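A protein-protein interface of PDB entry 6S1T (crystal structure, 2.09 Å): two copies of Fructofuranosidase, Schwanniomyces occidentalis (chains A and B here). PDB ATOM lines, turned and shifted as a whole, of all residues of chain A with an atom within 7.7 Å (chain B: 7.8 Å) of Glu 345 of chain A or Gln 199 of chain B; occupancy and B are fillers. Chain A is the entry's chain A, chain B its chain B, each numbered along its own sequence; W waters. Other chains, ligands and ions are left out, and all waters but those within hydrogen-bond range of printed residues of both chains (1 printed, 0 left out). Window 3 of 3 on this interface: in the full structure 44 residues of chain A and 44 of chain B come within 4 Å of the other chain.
The side-chain amide nitrogen of Gln 228 of chain B lies close to the side-chain amide nitrogen of Gln 199 of chain B (3.0 Å).
The side-chain carboxylate (OE2) of Glu 464 of chain A is in hydrogen-bond range of the side-chain hydroxyl (OH) of Tyr 462 of chain A (2.5 Å).
The side-chain amide oxygen (OD1) of Asn 343 of chain A is in hydrogen-bond range of the backbone NH (N) of Glu 345 of chain A (3.0 Å).
The side-chain amide oxygen (OD1) of Asn 343 of chain A is in hydrogen-bond range of the backbone NH (N) of Thr 346 of chain A (2.9 Å).
The side-chain hydroxyl (OH) of Tyr 201 of chain B lies within hydrogen-bond range of the backbone carbonyl oxygen (O) of Asn 227 of chain B (3.0 Å).
The side-chain amide oxygen (OE1) of Gln 228 of chain B lies close to the side-chain amide oxygen (OD1) of Asn 227 of chain B, at 3.5 Å.
Glu 345 of chain A touches just one residue of chain B: Gln 199.
Gln 199 of chain B touches just these residues of chain A: Asn 343, Ala 344, Glu 345 and Thr 346.
Ala 344 of chain A touches just one residue of chain B: Gln 199 (3.7 Å).
Of the printed residues of chain B, Tyr 462 of chain A touches Asn 227 and Pro 255.
Printed residues of chain A within 4 Å of Tyr 225 of chain B: Gln 348 (3.7 Å).
Printed residues of chain B within 4 Å of Thr 346 of chain A: Gln 199 (2.6 Å).
Of the printed residues of chain B, Gln 348 of chain A touches Tyr 225 (3.7 Å).
Printed residues of chain A within 4 Å of Asn 227 of chain B: Thr 342, Asn 343, Tyr 462 and Glu 464.
Ser 174 of chain B touches none of the printed residues of chain A.
Lys 202 of chain B touches none of the printed residues of chain A.
Water W1 lies within hydrogen-bond range of the side-chain carboxylate (OE2) of Glu 464 of chain A (2.8 Å), the backbone NH (N) of Ala 344 of chain A (2.9 Å) and the side-chain amide nitrogen (ND2) of Asn 227 of chain B (3.4 Å).
No position is printed for both chains.
Of the 12 pairs that touch across the chains among the printed residues, none has its exchanged pair printed and touching as well.
Ala 344 of chain A touches Gln 199 of chain B.
Tyr 225 of chain B touches Gln 348 of chain A (CE2 to OE1, 3.7 Å).
CE1 of Tyr 462 of chain A touches ND2 of Asn 227 of chain B, 3.5 Å away.
Tyr 462 of chain A touches Pro 255 of chain B.
The side-chain amide oxygen of Gln 199 of chain B sits at hydrogen-bond distance from the backbone NH of Glu 345 of chain A (3.4 Å).
The side-chain hydroxyl of Tyr 201 of chain B sits at hydrogen-bond distance from the side-chain hydroxyl of Thr 342 of chain A, 2.8 Å away.
The side-chain amide nitrogen (ND2) of Asn 227 of chain B lies within hydrogen-bond range of the side-chain carboxylate (OE2) of Glu 464 of chain A.
The backbone carbonyl oxygen (O) of Asn 227 of chain B sits at hydrogen-bond distance from the side-chain amide nitrogen (ND2) of Asn 343 of chain A (3.0 Å).
The side-chain amide nitrogen (ND2) of Asn 343 of chain A sits at hydrogen-bond distance from the backbone carbonyl oxygen (O) of Gln 199 of chain B.
OH of Tyr 201 of chain B sits at hydrogen-bond distance from ND2 of Asn 343 of chain A (3.3 Å).
OG1 of Thr 346 of chain A lies within hydrogen-bond range of O of Gln 199 of chain B, 2.6 Å away.
ND2 of Asn 227 of chain B sits at hydrogen-bond distance from O of Thr 342 of chain A (3.0 Å).
Of the 10 printed residues of chain A, 8 touch a printed residue of chain B.
Of the 19 printed residues of chain B, 5 touch a printed residue of chain A.
Hydrophobic or aromatic side chains of chain B that line the printed part of chain A: Tyr 201, Tyr 225 and Pro 255.
Among the printed residues, no Asp or Glu carboxylate lies within 4 Å of a Lys or Arg side-chain nitrogen of the other chain.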
ATOM      1  N   HIS A 341      13.316   9.932   4.651  1.00  0.00           N
ATOM      2  CA  HIS A 341      12.863   9.155   3.475  1.00  0.00           C
ATOM      3  C   HIS A 341      11.564   9.771   2.965  1.00  0.00           C
ATOM      4  O   HIS A 341      10.586   9.821   3.726  1.00  0.00           O
ATOM      5  CB  HIS A 341      12.734   7.655   3.798  1.00  0.00           C
ATOM      6  CG  HIS A 341      14.029   6.926   3.703  1.00  0.00           C
ATOM      7  ND1 HIS A 341      14.765   6.571   4.830  1.00  0.00           N
ATOM      8  CD2 HIS A 341      14.737   6.503   2.631  1.00  0.00           C
ATOM      9  CE1 HIS A 341      15.872   5.968   4.457  1.00  0.00           C
ATOM     10  NE2 HIS A 341      15.885   5.918   3.111  1.00  0.00           N
ATOM     11  N   THR A 342      11.581  10.266   1.728  1.00  0.00           N
ATOM     12  CA  THR A 342      10.359  10.700   1.005  1.00  0.00           C
ATOM     13  C   THR A 342       9.869   9.538   0.145  1.00  0.00           C
ATOM     14  O   THR A 342       8.715   9.571  -0.298  1.00  0.00           O
ATOM     15  CB  THR A 342      10.629  12.000   0.245  1.00  0.00           C
ATOM     16  OG1 THR A 342      11.711  11.786  -0.657  1.00  0.00           O
ATOM     17  CG2 THR A 342      10.968  13.127   1.192  1.00  0.00           C
ATOM     18  N   ASN A 343      10.746   8.568  -0.110  1.00  0.00           N
ATOM     19  CA  ASN A 343      10.368   7.252  -0.694  1.00  0.00           C
ATOM     20  C   ASN A 343      11.346   6.216  -0.121  1.00  0.00           C
ATOM     21  O   ASN A 343      12.245   6.613   0.635  1.00  0.00           O
ATOM     22  CB  ASN A 343      10.272   7.321  -2.224  1.00  0.00           C
ATOM     23  CG  ASN A 343      11.591   7.653  -2.893  1.00  0.00           C
ATOM     24  OD1 ASN A 343      12.626   7.098  -2.528  1.00  0.00           O
ATOM     25  ND2 ASN A 343      11.573   8.567  -3.854  1.00  0.00           N
ATOM     26  N   ALA A 344      11.159   4.939  -0.451  1.00  0.00           N
ATOM     27  CA  ALA A 344      11.945   3.808   0.096  1.00  0.00           C
ATOM     28  C   ALA A 344      13.442   4.000  -0.194  1.00  0.00           C
ATOM     29  O   ALA A 344      14.247   3.577   0.631  1.00  0.00           O
ATOM     30  CB  ALA A 344      11.434   2.507  -0.478  1.00  0.00           C
ATOM     31  N   GLU A 345      13.797   4.605  -1.323  1.00  0.00           N
ATOM     32  CA  GLU A 345      15.200   4.691  -1.814  1.00  0.00           C
ATOM     33  C   GLU A 345      15.890   5.975  -1.338  1.00  0.00           C
ATOM     34  O   GLU A 345      17.106   5.925  -1.149  1.00  0.00           O
ATOM     35  CB  GLU A 345      15.246   4.589  -3.344  1.00  0.00           C
ATOM     36  CG  GLU A 345      15.672   3.209  -3.831  1.00  0.00           C
ATOM     37  CD  GLU A 345      17.154   2.887  -3.658  1.00  0.00           C
ATOM     38  OE1 GLU A 345      17.984   3.620  -4.252  1.00  0.00           O
ATOM     39  OE2 GLU A 345      17.486   1.890  -2.951  1.00  0.00           O
ATOM     40  N   THR A 346      15.167   7.089  -1.209  1.00  0.00           N
ATOM     41  CA  THR A 346      15.769   8.450  -1.253  1.00  0.00           C
ATOM     42  C   THR A 346      15.377   9.266  -0.018  1.00  0.00           C
ATOM     43  O   THR A 346      14.194   9.293   0.341  1.00  0.00           O
ATOM     44  CB  THR A 346      15.358   9.187  -2.530  1.00  0.00           C
ATOM     45  OG1 THR A 346      15.734   8.354  -3.625  1.00  0.00           O
ATOM     46  CG2 THR A 346      15.977  10.560  -2.675  1.00  0.00           C
ATOM     47  N   LYS A 347      16.374   9.913   0.588  1.00  0.00           N
ATOM     48  CA  LYS A 347      16.221  10.879   1.704  1.00  0.00           C
ATOM     49  C   LYS A 347      16.341  12.299   1.149  1.00  0.00           C
ATOM     50  O   LYS A 347      17.110  12.501   0.204  1.00  0.00           O
ATOM     51  CB  LYS A 347      17.270  10.585   2.775  1.00  0.00           C
ATOM     52  CG  LYS A 347      17.010   9.302   3.555  1.00  0.00           C
ATOM     53  CD  LYS A 347      17.961   9.099   4.717  1.00  0.00           C
ATOM     54  CE  LYS A 347      19.305   8.564   4.283  1.00  0.00           C
ATOM     55  NZ  LYS A 347      20.074   8.093   5.456  1.00  0.00           N
ATOM     56  N   GLN A 348      15.533  13.220   1.675  1.00  0.00           N
ATOM     57  CA  GLN A 348      15.572  14.670   1.344  1.00  0.00           C
ATOM     58  C   GLN A 348      15.728  15.431   2.656  1.00  0.00           C
ATOM     59  O   GLN A 348      15.068  15.031   3.656  1.00  0.00           O
ATOM     60  CB  GLN A 348      14.285  15.139   0.663  1.00  0.00           C
ATOM     61  CG  GLN A 348      13.950  14.421  -0.629  1.00  0.00           C
ATOM     62  CD  GLN A 348      14.792  14.946  -1.765  1.00  0.00           C
ATOM     63  OE1 GLN A 348      14.670  16.093  -2.170  1.00  0.00           O
ATOM     64  NE2 GLN A 348      15.659  14.097  -2.294  1.00  0.00           N
ATOM     65  N   TYR A 462       0.469  11.391   2.964  1.00  0.00           N
ATOM     66  CA  TYR A 462       1.348  10.218   2.726  1.00  0.00           C
ATOM     67  C   TYR A 462       2.660  10.377   3.502  1.00  0.00           C
ATOM     68  O   TYR A 462       3.293  11.422   3.414  1.00  0.00           O
ATOM     69  CB  TYR A 462       1.655  10.052   1.239  1.00  0.00           C
ATOM     70  CG  TYR A 462       2.567   8.886   0.992  1.00  0.00           C
ATOM     71  CD1 TYR A 462       3.936   9.034   1.090  1.00  0.00           C
ATOM     72  CD2 TYR A 462       2.056   7.612   0.779  1.00  0.00           C
ATOM     73  CE1 TYR A 462       4.786   7.952   0.920  1.00  0.00           C
ATOM     74  CE2 TYR A 462       2.890   6.521   0.602  1.00  0.00           C
ATOM     75  CZ  TYR A 462       4.259   6.694   0.685  1.00  0.00           C
ATOM     76  OH  TYR A 462       5.106   5.638   0.527  1.00  0.00           O
ATOM     77  N   GLU A 464       6.369   7.952   4.508  1.00  0.00           N
ATOM     78  CA  GLU A 464       7.210   6.747   4.675  1.00  0.00           C
ATOM     79  C   GLU A 464       7.241   6.407   6.165  1.00  0.00           C
ATOM     80  O   GLU A 464       6.983   7.263   7.014  1.00  0.00           O
ATOM     81  CB  GLU A 464       8.595   7.007   4.103  1.00  0.00           C
ATOM     82  CG  GLU A 464       8.614   7.102   2.585  1.00  0.00           C
ATOM     83  CD  GLU A 464       8.367   5.784   1.867  1.00  0.00           C
ATOM     84  OE1 GLU A 464       8.958   4.758   2.291  1.00  0.00           O
ATOM     85  OE2 GLU A 464       7.564   5.776   0.885  1.00  0.00           O
ATOM     86  N   SER B 174      17.991  -1.437 -12.043  1.00  0.00           N
ATOM     87  CA  SER B 174      17.062  -0.746 -11.117  1.00  0.00           C
ATOM     88  C   SER B 174      15.675  -1.394 -11.183  1.00  0.00           C
ATOM     89  O   SER B 174      15.305  -1.960 -12.237  1.00  0.00           O
ATOM     90  CB  SER B 174      17.023   0.735 -11.402  1.00  0.00           C
ATOM     91  OG  SER B 174      15.940   1.355 -10.717  1.00  0.00           O
ATOM     92  N   ASN B 175      14.946  -1.323 -10.075  1.00  0.00           N
ATOM     93  CA  ASN B 175      13.540  -1.790  -9.976  1.00  0.00           C
ATOM     94  C   ASN B 175      12.601  -0.577  -9.912  1.00  0.00           C
ATOM     95  O   ASN B 175      11.419  -0.774  -9.618  1.00  0.00           O
ATOM     96  CB  ASN B 175      13.362  -2.742  -8.790  1.00  0.00           C
ATOM     97  CG  ASN B 175      13.563  -2.072  -7.446  1.00  0.00           C
ATOM     98  OD1 ASN B 175      14.212  -1.036  -7.348  1.00  0.00           O
ATOM     99  ND2 ASN B 175      13.012  -2.659  -6.398  1.00  0.00           N
ATOM    100  N   GLN B 176      13.115   0.626 -10.182  1.00  0.00           N
ATOM    101  CA  GLN B 176      12.353   1.902 -10.186  1.00  0.00           C
ATOM    102  C   GLN B 176      12.820   2.694 -11.401  1.00  0.00           C
ATOM    103  O   GLN B 176      13.599   3.655 -11.243  1.00  0.00           O
ATOM    104  CB  GLN B 176      12.583   2.671  -8.886  1.00  0.00           C
ATOM    105  CG  GLN B 176      12.049   1.948  -7.653  1.00  0.00           C
ATOM    106  CD  GLN B 176      10.542   1.886  -7.622  1.00  0.00           C
ATOM    107  OE1 GLN B 176       9.851   2.704  -8.227  1.00  0.00           O
ATOM    108  NE2 GLN B 176      10.014   0.919  -6.895  1.00  0.00           N
ATOM    109  N   PHE B 177      12.363   2.273 -12.574  1.00  0.00           N
ATOM    110  CA  PHE B 177      12.863   2.758 -13.881  1.00  0.00           C
ATOM    111  C   PHE B 177      11.830   2.430 -14.955  1.00  0.00           C
ATOM    112  O   PHE B 177      11.856   1.297 -15.473  1.00  0.00           O
ATOM    113  CB  PHE B 177      14.215   2.103 -14.161  1.00  0.00           C
ATOM    114  CG  PHE B 177      14.869   2.532 -15.443  1.00  0.00           C
ATOM    115  CD1 PHE B 177      15.069   3.872 -15.729  1.00  0.00           C
ATOM    116  CD2 PHE B 177      15.321   1.584 -16.342  1.00  0.00           C
ATOM    117  CE1 PHE B 177      15.719   4.256 -16.897  1.00  0.00           C
ATOM    118  CE2 PHE B 177      15.948   1.969 -17.513  1.00  0.00           C
ATOM    119  CZ  PHE B 177      16.152   3.300 -17.790  1.00  0.00           C
ATOM    120  N   ARG B 178      10.927   3.363 -15.249  1.00  0.00           N
ATOM    121  CA  ARG B 178       9.759   3.039 -16.110  1.00  0.00           C
ATOM    122  C   ARG B 178       9.133   4.248 -16.804  1.00  0.00           C
ATOM    123  O   ARG B 178       9.485   5.397 -16.472  1.00  0.00           O
ATOM    124  CB  ARG B 178       8.668   2.351 -15.283  1.00  0.00           C
ATOM    125  CG  ARG B 178       8.200   3.160 -14.079  1.00  0.00           C
ATOM    126  CD  ARG B 178       7.129   2.440 -13.285  1.00  0.00           C
ATOM    127  NE  ARG B 178       6.781   3.141 -12.052  1.00  0.00           N
ATOM    128  CZ  ARG B 178       7.488   3.094 -10.925  1.00  0.00           C
ATOM    129  NH1 ARG B 178       8.604   2.390 -10.866  1.00  0.00           N
ATOM    130  NH2 ARG B 178       7.087   3.771  -9.863  1.00  0.00           N
ATOM    131  N   SER B 196      11.239   7.770 -16.503  1.00  0.00           N
ATOM    132  CA  SER B 196      11.406   8.194 -15.094  1.00  0.00           C
ATOM    133  C   SER B 196      12.320   7.223 -14.333  1.00  0.00           C
ATOM    134  O   SER B 196      12.055   6.003 -14.347  1.00  0.00           O
ATOM    135  CB  SER B 196      10.089   8.396 -14.414  1.00  0.00           C
ATOM    136  OG  SER B 196       9.546   7.153 -13.984  1.00  0.00           O
ATOM    137  N   LYS B 197      13.353   7.777 -13.696  1.00  0.00           N
ATOM    138  CA  LYS B 197      14.091   7.130 -12.589  1.00  0.00           C
ATOM    139  C   LYS B 197      13.271   7.463 -11.340  1.00  0.00           C
ATOM    140  O   LYS B 197      13.575   8.472 -10.672  1.00  0.00           O
ATOM    141  CB  LYS B 197      15.534   7.642 -12.567  1.00  0.00           C
ATOM    142  CG  LYS B 197      16.557   6.707 -11.943  1.00  0.00           C
ATOM    143  CD  LYS B 197      16.522   5.307 -12.500  1.00  0.00           C
ATOM    144  CE  LYS B 197      17.483   4.367 -11.804  1.00  0.00           C
ATOM    145  NZ  LYS B 197      18.877   4.850 -11.909  1.00  0.00           N
ATOM    146  N   SER B 198      12.245   6.659 -11.083  1.00  0.00           N
ATOM    147  CA  SER B 198      11.028   7.088 -10.345  1.00  0.00           C
ATOM    148  C   SER B 198      11.395   7.592  -8.947  1.00  0.00           C
ATOM    149  O   SER B 198      10.947   8.696  -8.598  1.00  0.00           O
ATOM    150  CB  SER B 198      10.023   5.972 -10.305  1.00  0.00           C
ATOM    151  OG  SER B 198       9.774   5.510 -11.618  1.00  0.00           O
ATOM    152  N   GLN B 199      12.170   6.824  -8.178  1.00  0.00           N
ATOM    153  CA  GLN B 199      12.445   7.153  -6.750  1.00  0.00           C
ATOM    154  C   GLN B 199      13.714   7.999  -6.616  1.00  0.00           C
ATOM    155  O   GLN B 199      13.974   8.465  -5.501  1.00  0.00           O
ATOM    156  CB  GLN B 199      12.468   5.879  -5.916  1.00  0.00           C
ATOM    157  CG  GLN B 199      11.082   5.242  -5.890  1.00  0.00           C
ATOM    158  CD  GLN B 199      10.850   4.247  -4.783  1.00  0.00           C
ATOM    159  OE1 GLN B 199      11.740   3.942  -3.994  1.00  0.00           O
ATOM    160  NE2 GLN B 199       9.634   3.736  -4.721  1.00  0.00           N
ATOM    161  N   GLU B 200      14.408   8.292  -7.715  1.00  0.00           N
ATOM    162  CA  GLU B 200      15.516   9.283  -7.697  1.00  0.00           C
ATOM    163  C   GLU B 200      14.961  10.667  -8.032  1.00  0.00           C
ATOM    164  O   GLU B 200      15.748  11.618  -8.017  1.00  0.00           O
ATOM    165  CB  GLU B 200      16.633   8.900  -8.665  1.00  0.00           C
ATOM    166  CG  GLU B 200      17.470   7.733  -8.186  1.00  0.00           C
ATOM    167  CD  GLU B 200      18.608   7.382  -9.131  1.00  0.00           C
ATOM    168  OE1 GLU B 200      19.160   8.313  -9.758  1.00  0.00           O
ATOM    169  OE2 GLU B 200      18.942   6.189  -9.246  1.00  0.00           O
ATOM    170  N   TYR B 201      13.664  10.767  -8.356  1.00  0.00           N
ATOM    171  CA  TYR B 201      13.007  12.038  -8.749  1.00  0.00           C
ATOM    172  C   TYR B 201      13.769  12.635  -9.934  1.00  0.00           C
ATOM    173  O   TYR B 201      14.152  13.821  -9.908  1.00  0.00           O
ATOM    174  CB  TYR B 201      12.964  13.017  -7.576  1.00  0.00           C
ATOM    175  CG  TYR B 201      12.200  12.546  -6.364  1.00  0.00           C
ATOM    176  CD1 TYR B 201      10.823  12.366  -6.401  1.00  0.00           C
ATOM    177  CD2 TYR B 201      12.847  12.330  -5.155  1.00  0.00           C
ATOM    178  CE1 TYR B 201      10.120  11.948  -5.279  1.00  0.00           C
ATOM    179  CE2 TYR B 201      12.147  11.945  -4.020  1.00  0.00           C
ATOM    180  CZ  TYR B 201      10.780  11.766  -4.075  1.00  0.00           C
ATOM    181  OH  TYR B 201      10.112  11.383  -2.938  1.00  0.00           O
ATOM    182  N   LYS B 202      13.982  11.826 -10.970  1.00  0.00           N
ATOM    183  CA  LYS B 202      14.693  12.278 -12.192  1.00  0.00           C
ATOM    184  C   LYS B 202      13.933  11.821 -13.430  1.00  0.00           C
ATOM    185  O   LYS B 202      13.596  10.626 -13.506  1.00  0.00           O
ATOM    186  CB  LYS B 202      16.109  11.709 -12.194  1.00  0.00           C
ATOM    187  CG  LYS B 202      17.102  12.468 -11.331  1.00  0.00           C
ATOM    188  CD  LYS B 202      18.506  12.344 -11.854  1.00  0.00           C
ATOM    189  CE  LYS B 202      19.326  11.318 -11.119  1.00  0.00           C
ATOM    190  NZ  LYS B 202      20.478  11.923 -10.402  1.00  0.00           N
ATOM    191  N   TYR B 225       7.674  16.965  -5.968  1.00  0.00           N
ATOM    192  CA  TYR B 225       8.328  15.631  -6.017  1.00  0.00           C
ATOM    193  C   TYR B 225       7.324  14.540  -5.628  1.00  0.00           C
ATOM    194  O   TYR B 225       7.307  13.479  -6.268  1.00  0.00           O
ATOM    195  CB  TYR B 225       9.538  15.581  -5.081  1.00  0.00           C
ATOM    196  CG  TYR B 225      10.809  16.179  -5.630  1.00  0.00           C
ATOM    197  CD1 TYR B 225      10.802  17.067  -6.701  1.00  0.00           C
ATOM    198  CD2 TYR B 225      12.029  15.893  -5.036  1.00  0.00           C
ATOM    199  CE1 TYR B 225      11.975  17.632  -7.182  1.00  0.00           C
ATOM    200  CE2 TYR B 225      13.209  16.442  -5.508  1.00  0.00           C
ATOM    201  CZ  TYR B 225      13.184  17.312  -6.583  1.00  0.00           C
ATOM    202  OH  TYR B 225      14.357  17.863  -7.030  1.00  0.00           O
ATOM    203  N   ASN B 227       5.992  11.312  -3.838  1.00  0.00           N
ATOM    204  CA  ASN B 227       6.661  10.037  -3.467  1.00  0.00           C
ATOM    205  C   ASN B 227       7.570   9.563  -4.608  1.00  0.00           C
ATOM    206  O   ASN B 227       8.696   9.072  -4.310  1.00  0.00           O
ATOM    207  CB  ASN B 227       5.648   8.964  -3.086  1.00  0.00           C
ATOM    208  CG  ASN B 227       6.281   7.627  -2.761  1.00  0.00           C
ATOM    209  OD1 ASN B 227       6.100   6.659  -3.501  1.00  0.00           O
ATOM    210  ND2 ASN B 227       7.032   7.569  -1.674  1.00  0.00           N
ATOM    211  N   GLN B 228       7.135   9.699  -5.860  1.00  0.00           N
ATOM    212  CA  GLN B 228       7.884   9.189  -7.037  1.00  0.00           C
ATOM    213  C   GLN B 228       7.468   9.910  -8.317  1.00  0.00           C
ATOM    214  O   GLN B 228       6.301  10.320  -8.403  1.00  0.00           O
ATOM    215  CB  GLN B 228       7.516   7.743  -7.376  1.00  0.00           C
ATOM    216  CG  GLN B 228       7.514   6.772  -6.220  1.00  0.00           C
ATOM    217  CD  GLN B 228       6.864   5.474  -6.636  1.00  0.00           C
ATOM    218  OE1 GLN B 228       5.646   5.369  -6.719  1.00  0.00           O
ATOM    219  NE2 GLN B 228       7.678   4.475  -6.889  1.00  0.00           N
ATOM    220  N   TYR B 229       8.386   9.938  -9.283  1.00  0.00           N
ATOM    221  CA  TYR B 229       8.167  10.393 -10.674  1.00  0.00           C
ATOM    222  C   TYR B 229       7.643   9.235 -11.519  1.00  0.00           C
ATOM    223  O   TYR B 229       8.218   8.141 -11.427  1.00  0.00           O
ATOM    224  CB  TYR B 229       9.477  10.867 -11.289  1.00  0.00           C
ATOM    225  CG  TYR B 229       9.900  12.277 -10.972  1.00  0.00           C
ATOM    226  CD1 TYR B 229       9.368  13.008  -9.918  1.00  0.00           C
ATOM    227  CD2 TYR B 229      10.894  12.862 -11.738  1.00  0.00           C
ATOM    228  CE1 TYR B 229       9.776  14.312  -9.673  1.00  0.00           C
ATOM    229  CE2 TYR B 229      11.311  14.158 -11.507  1.00  0.00           C
ATOM    230  CZ  TYR B 229      10.744  14.888 -10.481  1.00  0.00           C
ATOM    231  OH  TYR B 229      11.212  16.149 -10.270  1.00  0.00           O
ATOM    232  N   GLU B 230       6.653   9.498 -12.374  1.00  0.00           N
ATOM    233  CA  GLU B 230       6.055   8.481 -13.273  1.00  0.00           C
ATOM    234  C   GLU B 230       5.608   9.131 -14.582  1.00  0.00           C
ATOM    235  O   GLU B 230       5.497  10.355 -14.617  1.00  0.00           O
ATOM    236  CB  GLU B 230       4.868   7.806 -12.578  1.00  0.00           C
ATOM    237  CG  GLU B 230       5.297   6.791 -11.541  1.00  0.00           C
ATOM    238  CD  GLU B 230       4.217   6.221 -10.648  1.00  0.00           C
ATOM    239  OE1 GLU B 230       4.579   5.412  -9.789  1.00  0.00           O
ATOM    240  OE2 GLU B 230       3.018   6.556 -10.840  1.00  0.00           O
ATOM    241  N   ASN B 254       2.877  10.042  -7.866  1.00  0.00           N
ATOM    242  CA  ASN B 254       1.950   9.223  -7.063  1.00  0.00           C
ATOM    243  C   ASN B 254       2.751   8.345  -6.119  1.00  0.00           C
ATOM    244  O   ASN B 254       3.742   7.772  -6.546  1.00  0.00           O
ATOM    245  CB  ASN B 254       1.084   8.317  -7.942  1.00  0.00           C
ATOM    246  CG  ASN B 254       0.194   7.442  -7.083  1.00  0.00           C
ATOM    247  OD1 ASN B 254      -0.629   7.951  -6.344  1.00  0.00           O
ATOM    248  ND2 ASN B 254       0.336   6.129  -7.178  1.00  0.00           N
ATOM    249  N   PRO B 255       2.345   8.188  -4.840  1.00  0.00           N
ATOM    250  CA  PRO B 255       1.392   9.087  -4.179  1.00  0.00           C
ATOM    251  C   PRO B 255       2.060  10.424  -3.799  1.00  0.00           C
ATOM    252  O   PRO B 255       3.131  10.726  -4.330  1.00  0.00           O
ATOM    253  CB  PRO B 255       0.955   8.262  -2.963  1.00  0.00           C
ATOM    254  CG  PRO B 255       2.185   7.441  -2.631  1.00  0.00           C
ATOM    255  CD  PRO B 255       2.751   7.066  -3.982  1.00  0.00           C
HETATM  256  O   HOH W   1       8.438   4.505  -1.458  1.00  0.00           O
